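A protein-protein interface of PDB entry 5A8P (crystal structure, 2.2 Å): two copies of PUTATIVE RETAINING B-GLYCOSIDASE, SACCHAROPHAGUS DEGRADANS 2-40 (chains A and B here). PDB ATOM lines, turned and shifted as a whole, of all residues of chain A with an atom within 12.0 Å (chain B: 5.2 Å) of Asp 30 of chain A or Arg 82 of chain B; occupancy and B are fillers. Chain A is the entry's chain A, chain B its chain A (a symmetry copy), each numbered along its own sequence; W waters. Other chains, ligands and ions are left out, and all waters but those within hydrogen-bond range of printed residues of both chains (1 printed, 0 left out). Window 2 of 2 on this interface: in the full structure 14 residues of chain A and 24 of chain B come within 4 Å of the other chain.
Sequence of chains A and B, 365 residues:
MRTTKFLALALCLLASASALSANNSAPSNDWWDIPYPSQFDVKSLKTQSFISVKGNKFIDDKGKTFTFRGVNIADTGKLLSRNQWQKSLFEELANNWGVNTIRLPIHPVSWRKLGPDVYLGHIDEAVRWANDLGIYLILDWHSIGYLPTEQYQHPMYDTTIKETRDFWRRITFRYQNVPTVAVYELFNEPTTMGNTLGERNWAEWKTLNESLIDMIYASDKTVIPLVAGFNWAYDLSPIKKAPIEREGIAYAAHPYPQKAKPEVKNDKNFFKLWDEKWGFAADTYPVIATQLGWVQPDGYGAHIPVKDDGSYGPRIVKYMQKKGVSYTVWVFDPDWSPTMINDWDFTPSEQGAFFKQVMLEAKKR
The guanidinium group (NH1) of Arg 82 of chain B is in hydrogen-bond range of the side-chain hydroxyl (OG) of Ser 81 of chain B, 2.9 Å away. The backbone carbonyl oxygen of Lys 78 of chain B is in hydrogen-bond range of the side-chain hydroxyl of Ser 81 of chain B, at 2.7 Å.
Of the 8 printed residues of chain A, 3 touch a printed residue of chain B.
No position is printed for both chains. Of the 5 pairs that touch across the chains among the printed residues, none has its exchanged pair printed and touching as well.
Among the printed residues, merely in contact across the chains: Trp 32 of chain A with Lys 78 of chain B (3.7 Å), Trp 32 of chain A with Ser 81 of chain B (3.7 Å) and Trp 32 of chain A with Arg 82 of chain B (3.7 Å).
Water W1 lies within hydrogen-bond range of O of Asn 29 of chain A (2.9 Å) and NZ of Lys 113 of chain B (3.0 Å).
The backbone carbonyl oxygen of Asn 29 of chain A sits at hydrogen-bond distance from the side-chain amino group of Lys 113 of chain B (2.7 Å). OD2 of Asp 30 of chain A is in salt-bridge range of NH2 of Arg 82 of chain B (2.9 Å).
Of the printed residues of chain B, Asp 30 of chain A touches Arg 82. No residue of chain A comes within 4 Å of Gln 84 of chain B. Of the printed residues of chain B, Trp 32 of chain A touches Lys 78 (3.7 Å), Ser 81 (3.7 Å) and Arg 82 (3.7 Å). Printed residues of chain A within 4 Å of Lys 113 of chain B: Asn 29. The nearest residue of chain A that does not touch Arg 82 of chain B is Asp 33 of chain A (5.6 Å). The nearest printed residue of chain B that does not touch Asn 29 of chain A is Arg 82 of chain B (6.7 Å).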
ATOM      1  N   ASN A  29       5.955 -17.933  -3.732  1.00  0.00           N
ATOM      2  CA  ASN A  29       6.266 -17.108  -2.521  1.00  0.00           C
ATOM      3  C   ASN A  29       5.535 -15.762  -2.508  1.00  0.00           C
ATOM      4  O   ASN A  29       5.188 -15.237  -1.436  1.00  0.00           O
ATOM      5  CB  ASN A  29       7.777 -16.855  -2.413  1.00  0.00           C
ATOM      6  CG  ASN A  29       8.561 -18.107  -2.069  1.00  0.00           C
ATOM      7  OD1 ASN A  29       8.203 -18.845  -1.150  1.00  0.00           O
ATOM      8  ND2 ASN A  29       9.647 -18.347  -2.802  1.00  0.00           N
ATOM      9  N   ASP A  30       5.327 -15.197  -3.696  1.00  0.00           N
ATOM     10  CA  ASP A  30       4.654 -13.922  -3.815  1.00  0.00           C
ATOM     11  C   ASP A  30       3.156 -14.185  -3.871  1.00  0.00           C
ATOM     12  O   ASP A  30       2.558 -14.318  -4.938  1.00  0.00           O
ATOM     13  CB  ASP A  30       5.143 -13.180  -5.044  1.00  0.00           C
ATOM     14  CG  ASP A  30       6.639 -12.945  -5.020  1.00  0.00           C
ATOM     15  OD1 ASP A  30       7.262 -13.168  -3.969  1.00  0.00           O
ATOM     16  OD2 ASP A  30       7.189 -12.545  -6.059  1.00  0.00           O
ATOM     17  N   TRP A  31       2.567 -14.282  -2.683  1.00  0.00           N
ATOM     18  CA  TRP A  31       1.138 -14.530  -2.537  1.00  0.00           C
ATOM     19  C   TRP A  31       0.298 -13.441  -3.202  1.00  0.00           C
ATOM     20  O   TRP A  31      -0.818 -13.693  -3.626  1.00  0.00           O
ATOM     21  CB  TRP A  31       0.772 -14.684  -1.056  1.00  0.00           C
ATOM     22  CG  TRP A  31       1.423 -13.674  -0.152  1.00  0.00           C
ATOM     23  CD1 TRP A  31       2.535 -13.863   0.609  1.00  0.00           C
ATOM     24  CD2 TRP A  31       1.009 -12.332   0.072  1.00  0.00           C
ATOM     25  NE1 TRP A  31       2.848 -12.719   1.290  1.00  0.00           N
ATOM     26  CE2 TRP A  31       1.917 -11.763   0.991  1.00  0.00           C
ATOM     27  CE3 TRP A  31      -0.050 -11.554  -0.397  1.00  0.00           C
ATOM     28  CZ2 TRP A  31       1.801 -10.448   1.447  1.00  0.00           C
ATOM     29  CZ3 TRP A  31      -0.156 -10.238   0.054  1.00  0.00           C
ATOM     30  CH2 TRP A  31       0.761  -9.705   0.970  1.00  0.00           C
ATOM     31  N   TRP A  32       0.848 -12.236  -3.321  1.00  0.00           N
ATOM     32  CA  TRP A  32       0.123 -11.143  -3.968  1.00  0.00           C
ATOM     33  C   TRP A  32       0.006 -11.324  -5.486  1.00  0.00           C
ATOM     34  O   TRP A  32      -0.728 -10.582  -6.127  1.00  0.00           O
ATOM     35  CB  TRP A  32       0.740  -9.775  -3.629  1.00  0.00           C
ATOM     36  CG  TRP A  32       2.175  -9.608  -4.011  1.00  0.00           C
ATOM     37  CD1 TRP A  32       2.663  -9.108  -5.185  1.00  0.00           C
ATOM     38  CD2 TRP A  32       3.313  -9.929  -3.208  1.00  0.00           C
ATOM     39  NE1 TRP A  32       4.030  -9.113  -5.165  1.00  0.00           N
ATOM     40  CE2 TRP A  32       4.459  -9.620  -3.966  1.00  0.00           C
ATOM     41  CE3 TRP A  32       3.476 -10.480  -1.935  1.00  0.00           C
ATOM     42  CZ2 TRP A  32       5.749  -9.826  -3.486  1.00  0.00           C
ATOM     43  CZ3 TRP A  32       4.759 -10.684  -1.456  1.00  0.00           C
ATOM     44  CH2 TRP A  32       5.881 -10.351  -2.232  1.00  0.00           C
ATOM     45  N   ASP A  33       0.729 -12.289  -6.053  1.00  0.00           N
ATOM     46  CA  ASP A  33       0.681 -12.578  -7.496  1.00  0.00           C
ATOM     47  C   ASP A  33      -0.135 -13.832  -7.803  1.00  0.00           C
ATOM     48  O   ASP A  33      -0.192 -14.272  -8.943  1.00  0.00           O
ATOM     49  CB  ASP A  33       2.104 -12.725  -8.076  1.00  0.00           C
ATOM     50  CG  ASP A  33       2.828 -11.387  -8.239  1.00  0.00           C
ATOM     51  OD1 ASP A  33       2.181 -10.328  -8.387  1.00  0.00           O
ATOM     52  OD2 ASP A  33       4.072 -11.391  -8.238  1.00  0.00           O
ATOM     53  N   ILE A  34      -0.771 -14.408  -6.792  1.00  0.00           N
ATOM     54  CA  ILE A  34      -1.657 -15.552  -6.999  1.00  0.00           C
ATOM     55  C   ILE A  34      -2.901 -15.102  -7.780  1.00  0.00           C
ATOM     56  O   ILE A  34      -3.615 -14.194  -7.337  1.00  0.00           O
ATOM     57  CB  ILE A  34      -2.072 -16.191  -5.667  1.00  0.00           C
ATOM     58  CG1 ILE A  34      -0.846 -16.819  -4.994  1.00  0.00           C
ATOM     59  CG2 ILE A  34      -3.156 -17.248  -5.887  1.00  0.00           C
ATOM     60  CD1 ILE A  34      -1.113 -17.318  -3.588  1.00  0.00           C
ATOM     61  N   PRO A  35      -3.163 -15.730  -8.943  1.00  0.00           N
ATOM     62  CA  PRO A  35      -4.246 -15.277  -9.823  1.00  0.00           C
ATOM     63  C   PRO A  35      -5.619 -15.390  -9.197  1.00  0.00           C
ATOM     64  O   PRO A  35      -5.833 -16.271  -8.385  1.00  0.00           O
ATOM     65  CB  PRO A  35      -4.177 -16.251 -11.016  1.00  0.00           C
ATOM     66  CG  PRO A  35      -2.802 -16.820 -10.969  1.00  0.00           C
ATOM     67  CD  PRO A  35      -2.425 -16.866  -9.522  1.00  0.00           C
ATOM     68  N   TYR A  36      -6.528 -14.497  -9.586  1.00  0.00           N
ATOM     69  CA  TYR A  36      -7.956 -14.689  -9.368  1.00  0.00           C
ATOM     70  C   TYR A  36      -8.464 -15.823 -10.261  1.00  0.00           C
ATOM     71  O   TYR A  36      -7.902 -16.066 -11.317  1.00  0.00           O
ATOM     72  CB  TYR A  36      -8.721 -13.393  -9.672  1.00  0.00           C
ATOM     73  CG  TYR A  36      -8.671 -12.411  -8.529  1.00  0.00           C
ATOM     74  CD1 TYR A  36      -7.627 -11.503  -8.410  1.00  0.00           C
ATOM     75  CD2 TYR A  36      -9.658 -12.413  -7.550  1.00  0.00           C
ATOM     76  CE1 TYR A  36      -7.577 -10.611  -7.343  1.00  0.00           C
ATOM     77  CE2 TYR A  36      -9.615 -11.539  -6.489  1.00  0.00           C
ATOM     78  CZ  TYR A  36      -8.573 -10.635  -6.389  1.00  0.00           C
ATOM     79  OH  TYR A  36      -8.529  -9.773  -5.323  1.00  0.00           O
ATOM     80  N   LYS B  78       5.892  -8.399   2.065  1.00  0.00           N
ATOM     81  CA  LYS B  78       6.231  -8.027   0.695  1.00  0.00           C
ATOM     82  C   LYS B  78       7.486  -7.157   0.693  1.00  0.00           C
ATOM     83  O   LYS B  78       8.397  -7.363  -0.113  1.00  0.00           O
ATOM     84  CB  LYS B  78       5.089  -7.289  -0.019  1.00  0.00           C
ATOM     85  CG  LYS B  78       5.542  -6.698  -1.351  1.00  0.00           C
ATOM     86  CD  LYS B  78       4.449  -5.994  -2.119  1.00  0.00           C
ATOM     87  CE  LYS B  78       4.980  -5.394  -3.429  1.00  0.00           C
ATOM     88  NZ  LYS B  78       6.059  -4.381  -3.239  1.00  0.00           N
ATOM     89  N   LEU B  79       7.534  -6.181   1.594  1.00  0.00           N
ATOM     90  CA  LEU B  79       8.683  -5.280   1.648  1.00  0.00           C
ATOM     91  C   LEU B  79       9.968  -6.015   2.054  1.00  0.00           C
ATOM     92  O   LEU B  79      11.029  -5.781   1.469  1.00  0.00           O
ATOM     93  CB  LEU B  79       8.397  -4.104   2.580  1.00  0.00           C
ATOM     94  CG  LEU B  79       7.324  -3.161   2.036  1.00  0.00           C
ATOM     95  CD1 LEU B  79       6.878  -2.190   3.114  1.00  0.00           C
ATOM     96  CD2 LEU B  79       7.813  -2.422   0.795  1.00  0.00           C
ATOM     97  N   LEU B  80       9.865  -6.902   3.045  1.00  0.00           N
ATOM     98  CA  LEU B  80      11.023  -7.686   3.470  1.00  0.00           C
ATOM     99  C   LEU B  80      11.594  -8.501   2.323  1.00  0.00           C
ATOM    100  O   LEU B  80      12.811  -8.621   2.216  1.00  0.00           O
ATOM    101  CB  LEU B  80      10.682  -8.648   4.608  1.00  0.00           C
ATOM    102  CG  LEU B  80      10.589  -8.017   5.985  1.00  0.00           C
ATOM    103  CD1 LEU B  80       9.881  -8.964   6.938  1.00  0.00           C
ATOM    104  CD2 LEU B  80      11.974  -7.656   6.510  1.00  0.00           C
ATOM    105  N   SER B  81      10.721  -9.067   1.484  1.00  0.00           N
ATOM    106  CA  SER B  81      11.165  -9.985   0.438  1.00  0.00           C
ATOM    107  C   SER B  81      12.053  -9.279  -0.584  1.00  0.00           C
ATOM    108  O   SER B  81      12.896  -9.917  -1.210  1.00  0.00           O
ATOM    109  CB  SER B  81       9.982 -10.658  -0.261  1.00  0.00           C
ATOM    110  OG  SER B  81       9.300  -9.740  -1.095  1.00  0.00           O
ATOM    111  N   ARG B  82      11.878  -7.970  -0.750  1.00  0.00           N
ATOM    112  CA  ARG B  82      12.739  -7.201  -1.652  1.00  0.00           C
ATOM    113  C   ARG B  82      13.670  -6.239  -0.889  1.00  0.00           C
ATOM    114  O   ARG B  82      14.161  -5.282  -1.463  1.00  0.00           O
ATOM    115  CB  ARG B  82      11.887  -6.439  -2.683  1.00  0.00           C
ATOM    116  CG  ARG B  82      10.905  -7.292  -3.493  1.00  0.00           C
ATOM    117  CD  ARG B  82      11.542  -8.566  -4.041  1.00  0.00           C
ATOM    118  NE  ARG B  82      10.803  -9.158  -5.165  1.00  0.00           N
ATOM    119  CZ  ARG B  82       9.807 -10.050  -5.074  1.00  0.00           C
ATOM    120  NH1 ARG B  82       9.362 -10.489  -3.900  1.00  0.00           N
ATOM    121  NH2 ARG B  82       9.248 -10.518  -6.187  1.00  0.00           N
ATOM    122  N   ASN B  83      13.911  -6.525   0.394  1.00  0.00           N
ATOM    123  CA  ASN B  83      14.755  -5.690   1.259  1.00  0.00           C
ATOM    124  C   ASN B  83      14.342  -4.215   1.307  1.00  0.00           C
ATOM    125  O   ASN B  83      15.184  -3.333   1.389  1.00  0.00           O
ATOM    126  CB  ASN B  83      16.232  -5.815   0.855  1.00  0.00           C
ATOM    127  CG  ASN B  83      16.702  -7.258   0.820  1.00  0.00           C
ATOM    128  OD1 ASN B  83      16.638  -7.966   1.824  1.00  0.00           O
ATOM    129  ND2 ASN B  83      17.166  -7.703  -0.342  1.00  0.00           N
ATOM    130  N   GLN B  84      13.039  -3.946   1.275  1.00  0.00           N
ATOM    131  CA  GLN B  84      12.557  -2.565   1.332  1.00  0.00           C
ATOM    132  C   GLN B  84      11.940  -2.215   2.688  1.00  0.00           C
ATOM    133  O   GLN B  84      11.464  -1.107   2.877  1.00  0.00           O
ATOM    134  CB  GLN B  84      11.563  -2.306   0.206  1.00  0.00           C
ATOM    135  CG  GLN B  84      12.155  -2.456  -1.195  1.00  0.00           C
ATOM    136  CD  GLN B  84      13.191  -1.394  -1.544  1.00  0.00           C
ATOM    137  OE1 GLN B  84      13.236  -0.319  -0.948  1.00  0.00           O
ATOM    138  NE2 GLN B  84      14.026  -1.697  -2.528  1.00  0.00           N
ATOM    139  N   LYS B 113       2.433 -16.620   7.150  1.00  0.00           N
ATOM    140  CA  LYS B 113       3.691 -17.009   6.520  1.00  0.00           C
ATOM    141  C   LYS B 113       4.916 -16.634   7.353  1.00  0.00           C
ATOM    142  O   LYS B 113       5.817 -17.444   7.514  1.00  0.00           O
ATOM    143  CB  LYS B 113       3.803 -16.403   5.127  1.00  0.00           C
ATOM    144  CG  LYS B 113       4.955 -16.968   4.324  1.00  0.00           C
ATOM    145  CD  LYS B 113       4.859 -16.561   2.860  1.00  0.00           C
ATOM    146  CE  LYS B 113       5.958 -17.224   2.045  1.00  0.00           C
ATOM    147  NZ  LYS B 113       6.155 -16.547   0.735  1.00  0.00           N
HETATM  148  O   HOH W   1       6.578 -13.571   0.443  1.00  0.00           O
